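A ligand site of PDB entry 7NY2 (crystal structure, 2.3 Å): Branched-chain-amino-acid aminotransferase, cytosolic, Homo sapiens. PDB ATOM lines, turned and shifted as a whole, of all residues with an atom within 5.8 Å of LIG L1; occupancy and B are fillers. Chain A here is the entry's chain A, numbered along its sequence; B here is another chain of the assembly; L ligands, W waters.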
ATOM      1  N   PHE A  52      -4.261   3.353  -4.634  1.00  0.00           N
ATOM      2  CA  PHE A  52      -3.850   4.738  -4.933  1.00  0.00           C
ATOM      3  C   PHE A  52      -5.032   5.553  -5.490  1.00  0.00           C
ATOM      4  O   PHE A  52      -5.654   5.141  -6.524  1.00  0.00           O
ATOM      5  CB  PHE A  52      -2.731   4.732  -5.963  1.00  0.00           C
ATOM      6  CG  PHE A  52      -2.361   6.141  -6.301  1.00  0.00           C
ATOM      7  CD1 PHE A  52      -1.693   6.916  -5.368  1.00  0.00           C
ATOM      8  CD2 PHE A  52      -2.760   6.708  -7.506  1.00  0.00           C
ATOM      9  CE1 PHE A  52      -1.366   8.236  -5.649  1.00  0.00           C
ATOM     10  CE2 PHE A  52      -2.443   8.030  -7.777  1.00  0.00           C
ATOM     11  CZ  PHE A  52      -1.749   8.784  -6.855  1.00  0.00           C
ATOM     12  N   PHE A  98      -1.683  20.365 -12.457  1.00  0.00           N
ATOM     13  CA  PHE A  98      -1.728  19.668 -11.141  1.00  0.00           C
ATOM     14  C   PHE A  98      -0.299  19.535 -10.594  1.00  0.00           C
ATOM     15  O   PHE A  98       0.665  19.899 -11.276  1.00  0.00           O
ATOM     16  CB  PHE A  98      -2.371  18.281 -11.242  1.00  0.00           C
ATOM     17  CG  PHE A  98      -1.631  17.289 -12.129  1.00  0.00           C
ATOM     18  CD1 PHE A  98      -1.653  17.417 -13.508  1.00  0.00           C
ATOM     19  CD2 PHE A  98      -0.933  16.226 -11.582  1.00  0.00           C
ATOM     20  CE1 PHE A  98      -0.977  16.530 -14.319  1.00  0.00           C
ATOM     21  CE2 PHE A  98      -0.240  15.344 -12.418  1.00  0.00           C
ATOM     22  CZ  PHE A  98      -0.272  15.479 -13.778  1.00  0.00           C
ATOM     23  N   LYS A 102       3.680  14.311  -0.928  1.00  0.00           N
ATOM     24  CA  LYS A 102       3.195  13.500   0.229  1.00  0.00           C
ATOM     25  C   LYS A 102       3.497  14.189   1.583  1.00  0.00           C
ATOM     26  O   LYS A 102       4.374  15.106   1.667  1.00  0.00           O
ATOM     27  CB  LYS A 102       3.800  12.098   0.179  1.00  0.00           C
ATOM     28  CG  LYS A 102       3.616  11.365  -1.155  1.00  0.00           C
ATOM     29  CD  LYS A 102       4.152   9.958  -1.172  1.00  0.00           C
ATOM     30  CE  LYS A 102       3.490   9.116  -2.250  1.00  0.00           C
ATOM     31  NZ  LYS A 102       3.827   7.670  -2.156  1.00  0.00           N
ATOM     32  N   TYR A 164      -1.340  11.356   0.157  1.00  0.00           N
ATOM     33  CA  TYR A 164      -1.025  12.033  -1.120  1.00  0.00           C
ATOM     34  C   TYR A 164      -1.741  13.380  -1.082  1.00  0.00           C
ATOM     35  O   TYR A 164      -2.932  13.410  -0.672  1.00  0.00           O
ATOM     36  CB  TYR A 164      -1.438  11.187  -2.328  1.00  0.00           C
ATOM     37  CG  TYR A 164      -0.987  11.649  -3.686  1.00  0.00           C
ATOM     38  CD1 TYR A 164       0.340  11.578  -4.100  1.00  0.00           C
ATOM     39  CD2 TYR A 164      -1.906  12.071  -4.630  1.00  0.00           C
ATOM     40  CE1 TYR A 164       0.736  11.961  -5.374  1.00  0.00           C
ATOM     41  CE2 TYR A 164      -1.534  12.461  -5.920  1.00  0.00           C
ATOM     42  CZ  TYR A 164      -0.200  12.417  -6.291  1.00  0.00           C
ATOM     43  OH  TYR A 164       0.184  12.764  -7.580  1.00  0.00           O
ATOM     44  N   ARG A 166      -2.820  16.615  -3.595  1.00  0.00           N
ATOM     45  CA  ARG A 166      -3.189  16.854  -5.020  1.00  0.00           C
ATOM     46  C   ARG A 166      -3.713  18.282  -5.162  1.00  0.00           C
ATOM     47  O   ARG A 166      -4.924  18.479  -5.274  1.00  0.00           O
ATOM     48  CB  ARG A 166      -4.191  15.806  -5.519  1.00  0.00           C
ATOM     49  CG  ARG A 166      -4.686  16.009  -6.956  1.00  0.00           C
ATOM     50  CD  ARG A 166      -3.639  16.420  -7.965  1.00  0.00           C
ATOM     51  NE  ARG A 166      -2.710  15.331  -8.197  1.00  0.00           N
ATOM     52  CZ  ARG A 166      -2.815  14.425  -9.183  1.00  0.00           C
ATOM     53  NH1 ARG A 166      -3.798  14.460 -10.059  1.00  0.00           N
ATOM     54  NH2 ARG A 166      -1.908  13.487  -9.304  1.00  0.00           N
ATOM     55  N   TYR A 196       4.159   1.352  -2.636  1.00  0.00           N
ATOM     56  CA  TYR A 196       4.035   1.147  -4.103  1.00  0.00           C
ATOM     57  C   TYR A 196       3.874  -0.346  -4.379  1.00  0.00           C
ATOM     58  O   TYR A 196       2.879  -0.722  -5.046  1.00  0.00           O
ATOM     59  CB  TYR A 196       5.216   1.751  -4.867  1.00  0.00           C
ATOM     60  CG  TYR A 196       4.994   1.857  -6.359  1.00  0.00           C
ATOM     61  CD1 TYR A 196       4.236   2.880  -6.877  1.00  0.00           C
ATOM     62  CD2 TYR A 196       5.509   0.923  -7.246  1.00  0.00           C
ATOM     63  CE1 TYR A 196       4.021   2.996  -8.250  1.00  0.00           C
ATOM     64  CE2 TYR A 196       5.300   1.018  -8.618  1.00  0.00           C
ATOM     65  CZ  TYR A 196       4.555   2.072  -9.130  1.00  0.00           C
ATOM     66  OH  TYR A 196       4.290   2.269 -10.457  1.00  0.00           O
ATOM     67  N   LYS A 225       3.812  20.283 -15.632  1.00  0.00           N
ATOM     68  CA  LYS A 225       2.786  19.263 -15.237  1.00  0.00           C
ATOM     69  C   LYS A 225       1.409  19.765 -15.684  1.00  0.00           C
ATOM     70  O   LYS A 225       0.560  20.020 -14.816  1.00  0.00           O
ATOM     71  CB  LYS A 225       2.895  18.892 -13.746  1.00  0.00           C
ATOM     72  CG  LYS A 225       3.145  17.403 -13.487  1.00  0.00           C
ATOM     73  CD  LYS A 225       3.530  17.077 -12.036  1.00  0.00           C
ATOM     74  CE  LYS A 225       3.505  15.587 -11.702  1.00  0.00           C
ATOM     75  NZ  LYS A 225       4.690  14.843 -12.195  1.00  0.00           N
ATOM     76  N   TYR A 230      -0.773  14.281 -20.557  1.00  0.00           N
ATOM     77  CA  TYR A 230      -1.089  12.955 -19.931  1.00  0.00           C
ATOM     78  C   TYR A 230      -2.231  12.256 -20.683  1.00  0.00           C
ATOM     79  O   TYR A 230      -2.219  11.016 -20.800  1.00  0.00           O
ATOM     80  CB  TYR A 230      -1.373  13.181 -18.421  1.00  0.00           C
ATOM     81  CG  TYR A 230      -0.153  13.760 -17.758  1.00  0.00           C
ATOM     82  CD1 TYR A 230       0.881  12.936 -17.365  1.00  0.00           C
ATOM     83  CD2 TYR A 230       0.045  15.128 -17.686  1.00  0.00           C
ATOM     84  CE1 TYR A 230       2.060  13.467 -16.849  1.00  0.00           C
ATOM     85  CE2 TYR A 230       1.216  15.679 -17.193  1.00  0.00           C
ATOM     86  CZ  TYR A 230       2.227  14.840 -16.770  1.00  0.00           C
ATOM     87  OH  TYR A 230       3.398  15.349 -16.289  1.00  0.00           O
ATOM     88  N   GLN A 237      -0.223   2.886 -22.897  1.00  0.00           N
ATOM     89  CA  GLN A 237      -0.162   2.086 -21.656  1.00  0.00           C
ATOM     90  C   GLN A 237      -1.053   0.866 -21.782  1.00  0.00           C
ATOM     91  O   GLN A 237      -0.591  -0.205 -21.348  1.00  0.00           O
ATOM     92  CB  GLN A 237      -0.660   2.840 -20.420  1.00  0.00           C
ATOM     93  CG  GLN A 237      -0.741   1.954 -19.164  1.00  0.00           C
ATOM     94  CD  GLN A 237       0.620   1.574 -18.636  1.00  0.00           C
ATOM     95  OE1 GLN A 237       1.616   2.141 -19.016  1.00  0.00           O
ATOM     96  NE2 GLN A 237       0.658   0.596 -17.744  1.00  0.00           N
ATOM     97  N   GLN A 246       4.553  -3.391 -17.824  1.00  0.00           N
ATOM     98  CA  GLN A 246       3.933  -2.647 -16.705  1.00  0.00           C
ATOM     99  C   GLN A 246       4.076  -1.141 -16.949  1.00  0.00           C
ATOM    100  O   GLN A 246       3.366  -0.375 -16.314  1.00  0.00           O
ATOM    101  CB  GLN A 246       4.595  -2.997 -15.372  1.00  0.00           C
ATOM    102  CG  GLN A 246       4.186  -4.327 -14.762  1.00  0.00           C
ATOM    103  CD  GLN A 246       4.999  -5.497 -15.264  1.00  0.00           C
ATOM    104  OE1 GLN A 246       6.223  -5.430 -15.350  1.00  0.00           O
ATOM    105  NE2 GLN A 246       4.319  -6.571 -15.616  1.00  0.00           N
ATOM    106  N   GLN A 247       4.981  -0.701 -17.823  1.00  0.00           N
ATOM    107  CA  GLN A 247       5.146   0.729 -18.174  1.00  0.00           C
ATOM    108  C   GLN A 247       5.589   0.847 -19.631  1.00  0.00           C
ATOM    109  O   GLN A 247       6.022  -0.176 -20.202  1.00  0.00           O
ATOM    110  CB  GLN A 247       6.193   1.401 -17.287  1.00  0.00           C
ATOM    111  CG  GLN A 247       5.864   1.441 -15.805  1.00  0.00           C
ATOM    112  CD  GLN A 247       4.790   2.406 -15.368  1.00  0.00           C
ATOM    113  OE1 GLN A 247       4.577   3.484 -15.915  1.00  0.00           O
ATOM    114  NE2 GLN A 247       4.083   2.018 -14.327  1.00  0.00           N
ATOM    115  N   GLY A 262       7.196   5.768 -18.245  1.00  0.00           N
ATOM    116  CA  GLY A 262       5.815   6.145 -17.828  1.00  0.00           C
ATOM    117  C   GLY A 262       5.777   7.614 -17.393  1.00  0.00           C
ATOM    118  O   GLY A 262       6.184   8.488 -18.179  1.00  0.00           O
ATOM    119  N   THR A 263       5.335   7.872 -16.160  1.00  0.00           N
ATOM    120  CA  THR A 263       5.429   9.177 -15.457  1.00  0.00           C
ATOM    121  C   THR A 263       6.534   9.140 -14.379  1.00  0.00           C
ATOM    122  O   THR A 263       6.314   9.749 -13.288  1.00  0.00           O
ATOM    123  CB  THR A 263       4.064   9.494 -14.814  1.00  0.00           C
ATOM    124  OG1 THR A 263       3.723   8.471 -13.864  1.00  0.00           O
ATOM    125  CG2 THR A 263       2.962   9.612 -15.833  1.00  0.00           C
ATOM    126  N   MET A 264       7.666   8.465 -14.651  1.00  0.00           N
ATOM    127  CA  MET A 264       8.912   8.447 -13.814  1.00  0.00           C
ATOM    128  C   MET A 264      10.124   8.881 -14.643  1.00  0.00           C
ATOM    129  O   MET A 264      10.182   8.526 -15.824  1.00  0.00           O
ATOM    130  CB  MET A 264       9.195   7.046 -13.247  1.00  0.00           C
ATOM    131  CG  MET A 264       7.936   6.406 -12.651  1.00  0.00           C
ATOM    132  SD  MET A 264       8.127   4.917 -11.633  1.00  0.00           S
ATOM    133  CE  MET A 264       8.961   3.810 -12.760  1.00  0.00           C
ATOM    134  N   THR A 336       7.675  10.534  -7.155  1.00  0.00           N
ATOM    135  CA  THR A 336       6.950  10.551  -5.867  1.00  0.00           C
ATOM    136  C   THR A 336       6.298   9.184  -5.650  1.00  0.00           C
ATOM    137  O   THR A 336       6.225   8.726  -4.486  1.00  0.00           O
ATOM    138  CB  THR A 336       5.966  11.718  -5.782  1.00  0.00           C
ATOM    139  OG1 THR A 336       6.829  12.851  -5.645  1.00  0.00           O
ATOM    140  CG2 THR A 336       5.004  11.651  -4.612  1.00  0.00           C
ATOM    141  N   ALA A 337       5.912   8.540  -6.748  1.00  0.00           N
ATOM    142  CA  ALA A 337       5.141   7.274  -6.729  1.00  0.00           C
ATOM    143  C   ALA A 337       5.925   6.180  -6.012  1.00  0.00           C
ATOM    144  O   ALA A 337       5.449   5.665  -4.991  1.00  0.00           O
ATOM    145  CB  ALA A 337       4.834   6.880  -8.151  1.00  0.00           C
ATOM    146  N   TYR B  93      -5.927  15.001 -16.225  1.00  0.00           N
ATOM    147  CA  TYR B  93      -5.094  14.402 -17.296  1.00  0.00           C
ATOM    148  C   TYR B  93      -5.714  14.617 -18.701  1.00  0.00           C
ATOM    149  O   TYR B  93      -5.435  13.865 -19.678  1.00  0.00           O
ATOM    150  CB  TYR B  93      -4.832  12.912 -17.024  1.00  0.00           C
ATOM    151  CG  TYR B  93      -4.504  12.560 -15.586  1.00  0.00           C
ATOM    152  CD1 TYR B  93      -3.443  13.150 -14.916  1.00  0.00           C
ATOM    153  CD2 TYR B  93      -5.271  11.649 -14.870  1.00  0.00           C
ATOM    154  CE1 TYR B  93      -3.163  12.865 -13.585  1.00  0.00           C
ATOM    155  CE2 TYR B  93      -5.010  11.358 -13.537  1.00  0.00           C
ATOM    156  CZ  TYR B  93      -3.959  11.972 -12.904  1.00  0.00           C
ATOM    157  OH  TYR B  93      -3.710  11.673 -11.602  1.00  0.00           O
ATOM    158  N   LEU B 176      -7.507   9.364  -9.139  1.00  0.00           N
ATOM    159  CA  LEU B 176      -6.289  10.089  -9.579  1.00  0.00           C
ATOM    160  C   LEU B 176      -5.364   9.148 -10.334  1.00  0.00           C
ATOM    161  O   LEU B 176      -4.322   9.600 -10.797  1.00  0.00           O
ATOM    162  CB  LEU B 176      -5.566  10.614  -8.338  1.00  0.00           C
ATOM    163  CG  LEU B 176      -6.397  11.379  -7.311  1.00  0.00           C
ATOM    164  CD1 LEU B 176      -5.478  11.936  -6.235  1.00  0.00           C
ATOM    165  CD2 LEU B 176      -7.201  12.488  -7.969  1.00  0.00           C
ATOM    166  N   GLY B 177      -5.651   7.854 -10.349  1.00  0.00           N
ATOM    167  CA  GLY B 177      -4.800   6.916 -11.099  1.00  0.00           C
ATOM    168  C   GLY B 177      -4.837   7.260 -12.572  1.00  0.00           C
ATOM    169  O   GLY B 177      -5.944   7.521 -13.077  1.00  0.00           O
ATOM    170  N   VAL B 178      -3.678   7.298 -13.249  1.00  0.00           N
ATOM    171  CA  VAL B 178      -3.619   7.558 -14.716  1.00  0.00           C
ATOM    172  C   VAL B 178      -4.034   6.274 -15.449  1.00  0.00           C
ATOM    173  O   VAL B 178      -3.218   5.350 -15.492  1.00  0.00           O
ATOM    174  CB  VAL B 178      -2.213   8.035 -15.112  1.00  0.00           C
ATOM    175  CG1 VAL B 178      -2.091   8.321 -16.612  1.00  0.00           C
ATOM    176  CG2 VAL B 178      -1.784   9.228 -14.272  1.00  0.00           C
ATOM    177  N   LYS B 179      -5.271   6.182 -15.954  1.00  0.00           N
ATOM    178  CA  LYS B 179      -5.737   4.968 -16.683  1.00  0.00           C
ATOM    179  C   LYS B 179      -7.028   5.192 -17.509  1.00  0.00           C
ATOM    180  O   LYS B 179      -7.581   6.277 -17.525  1.00  0.00           O
ATOM    181  CB  LYS B 179      -5.914   3.825 -15.681  1.00  0.00           C
ATOM    182  CG  LYS B 179      -7.263   3.721 -14.992  1.00  0.00           C
ATOM    183  CD  LYS B 179      -7.837   4.983 -14.444  1.00  0.00           C
ATOM    184  CE  LYS B 179      -8.761   4.746 -13.260  1.00  0.00           C
ATOM    185  NZ  LYS B 179      -9.627   3.546 -13.407  1.00  0.00           N
HETATM  186  C1  LIG L   1       0.887   5.571  -9.204  1.00  0.00           C
HETATM  187  C2  LIG L   1       1.114   6.348  -8.073  1.00  0.00           C
HETATM  188  C3  LIG L   1       1.453   7.704  -8.213  1.00  0.00           C
HETATM  189  C4  LIG L   1       0.560   4.205  -9.069  1.00  0.00           C
HETATM  190  C5  LIG L   1       0.470   3.615  -7.813  1.00  0.00           C
HETATM  191  C6  LIG L   1       1.046   5.755  -6.814  1.00  0.00           C
HETATM  192  N1  LIG L   1       0.785   5.398 -11.631  1.00  0.00           N
HETATM  193  C7  LIG L   1       1.704  10.454 -10.644  1.00  0.00           C
HETATM  194  C8  LIG L   1       0.282  11.468 -12.347  1.00  0.00           C
HETATM  195  C9  LIG L   1       2.830  11.042 -11.254  1.00  0.00           C
HETATM  196  C10 LIG L   1      -0.852  10.068 -10.606  1.00  0.00           C
HETATM  197  C11 LIG L   1       1.835   4.593 -12.065  1.00  0.00           C
HETATM  198  C12 LIG L   1       0.544   3.850 -13.940  1.00  0.00           C
HETATM  199  C13 LIG L   1       0.423  10.684 -11.211  1.00  0.00           C
HETATM  200  C14 LIG L   1       1.415  12.035 -12.957  1.00  0.00           C
HETATM  201  C15 LIG L   1       2.690  11.822 -12.399  1.00  0.00           C
HETATM  202  O1  LIG L   1       1.902   9.686  -9.513  1.00  0.00           O
HETATM  203  C16 LIG L   1       1.569   8.316  -9.467  1.00  0.00           C
HETATM  204  C17 LIG L   1       1.324   7.528 -10.606  1.00  0.00           C
HETATM  205  C18 LIG L   1       1.699   8.464  -7.037  1.00  0.00           C
HETATM  206  N2  LIG L   1       1.904   9.104  -6.118  1.00  0.00           N
HETATM  207  C19 LIG L   1       0.713   4.406  -6.689  1.00  0.00           C
HETATM  208  C20 LIG L   1       0.984   6.168 -10.475  1.00  0.00           C
HETATM  209  C21 LIG L   1      -0.398   5.413 -12.360  1.00  0.00           C
HETATM  210  O2  LIG L   1      -1.331   6.109 -11.997  1.00  0.00           O
HETATM  211  C22 LIG L   1      -0.524   4.640 -13.522  1.00  0.00           C
HETATM  212  C23 LIG L   1       0.505   2.960 -15.192  1.00  0.00           C
HETATM  213  F1  LIG L   1      -0.637   3.035 -15.861  1.00  0.00           F
HETATM  214  F2  LIG L   1       1.506   3.298 -16.006  1.00  0.00           F
HETATM  215  F3  LIG L   1       0.660   1.714 -14.762  1.00  0.00           F
HETATM  216  N3  LIG L   1       1.707   3.839 -13.191  1.00  0.00           N
HETATM  217  O3  LIG L   1       2.883   4.542 -11.449  1.00  0.00           O
HETATM  218  N1  LG2 L   2       7.886  12.288 -15.102  1.00  0.00           N
HETATM  219  C1  LG2 L   2       6.710  12.870 -15.375  1.00  0.00           C
HETATM  220  C2  LG2 L   2       6.280  12.957 -16.802  1.00  0.00           C
HETATM  221  C3  LG2 L   2       5.917  13.386 -14.349  1.00  0.00           C
HETATM  222  O1  LG2 L   2       4.741  13.958 -14.661  1.00  0.00           O
HETATM  223  C4  LG2 L   2       6.344  13.287 -13.006  1.00  0.00           C
HETATM  224  C5  LG2 L   2       5.477  13.848 -11.963  1.00  0.00           C
HETATM  225  C6  LG2 L   2       7.581  12.665 -12.754  1.00  0.00           C
HETATM  226  C7  LG2 L   2       8.297  12.187 -13.817  1.00  0.00           C
HETATM  227  C8  LG2 L   2       8.127  12.489 -11.363  1.00  0.00           C
HETATM  228  O2  LG2 L   2       8.277  13.771 -10.691  1.00  0.00           O
HETATM  229  P1  LG2 L   2       8.415  13.790  -9.054  1.00  0.00           P
HETATM  230  O3  LG2 L   2       7.258  12.959  -8.497  1.00  0.00           O
HETATM  231  O4  LG2 L   2       8.306  15.244  -8.774  1.00  0.00           O
HETATM  232  O5  LG2 L   2       9.738  13.185  -8.715  1.00  0.00           O
HETATM  233  O   HOH W   1       2.892   5.508  -4.008  1.00  0.00           O
HETATM  234  O   HOH W   2       2.820  12.431  -8.272  1.00  0.00           O
HETATM  235  O   HOH W   3       3.588   3.776 -18.545  1.00  0.00           O
HETATM  236  O   HOH W   4      -2.545   4.820 -17.816  1.00  0.00           O
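NE2 of Gln 247 sits close to N3 of LIG L1, 3.2 Å away. The backbone NH (N) of Thr 336 lies within hydrogen-bond range of an oxygen (O3) of LG2 L2. An oxygen (O3) of LG2 L2 is in hydrogen-bond range of the side-chain hydroxyl of Thr 336, 2.9 Å away. The backbone NH (N) of Val 178 of chain B sits at hydrogen-bond distance from an oxygen (O2) of LIG L1 (2.9 Å). O3 of LIG L1 sits at hydrogen-bond distance from OH of Tyr 196 (2.9 Å). The side-chain hydroxyl (OH) of Tyr 230 is in hydrogen-bond range of an oxygen (O1) of LG2 L2. The side-chain amino group (NZ) of Lys 225 is bonded to a carbon (C5) of LG2 L2 (1.3 Å).
The backbone carbonyl oxygen (O) of Lys 225 is in hydrogen-bond range of the backbone NH (N) of Phe 98 (3.3 Å). The side-chain hydroxyl of Tyr 164 is in hydrogen-bond range of the guanidinium group of Arg 166 (2.8 Å). The guanidinium group of Arg 166 sits at hydrogen-bond distance from the side-chain hydroxyl of Tyr 93 of chain B (3.2 Å). NE2 of Gln 237 sits at hydrogen-bond distance from O of Gln 246 (3.2 Å).
The side-chain amide nitrogen (NE2) of Gln 237 lies close to a fluorine (F3) of LIG L1, at 3.2 Å. Residues that only touch LIG L1: Phe 52 (3.3 Å), Phe 98 (3.7 Å), Tyr 164 (3.2 Å), Arg 166 (3.8 Å), Lys 225 (3.6 Å), Gln 246 (3.8 Å), Thr 263 (3.6 Å), Ala 337 (3.5 Å), Tyr 93 of chain B (3.4 Å), Leu 176 of chain B (3.5 Å) and Gly 177 of chain B (3.7 Å). Hydrophobic or aromatic side chains within 4 Å of LIG L1: Phe 52, Phe 98, Tyr 164, Tyr 196, Ala 337, Tyr 93 of chain B and Val 178 of chain B.
Water W2 lies within hydrogen-bond range of OH of Tyr 164 (2.7 Å) and O1 of LIG L1 (3.1 Å). Water W3 bridges the side-chain amide oxygen of Gln 237 (2.6 Å) and the side-chain amide oxygen of Gln 247 (2.8 Å). Water W1 lies within hydrogen-bond range of O of Ala 337 and NZ of Lys 102.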
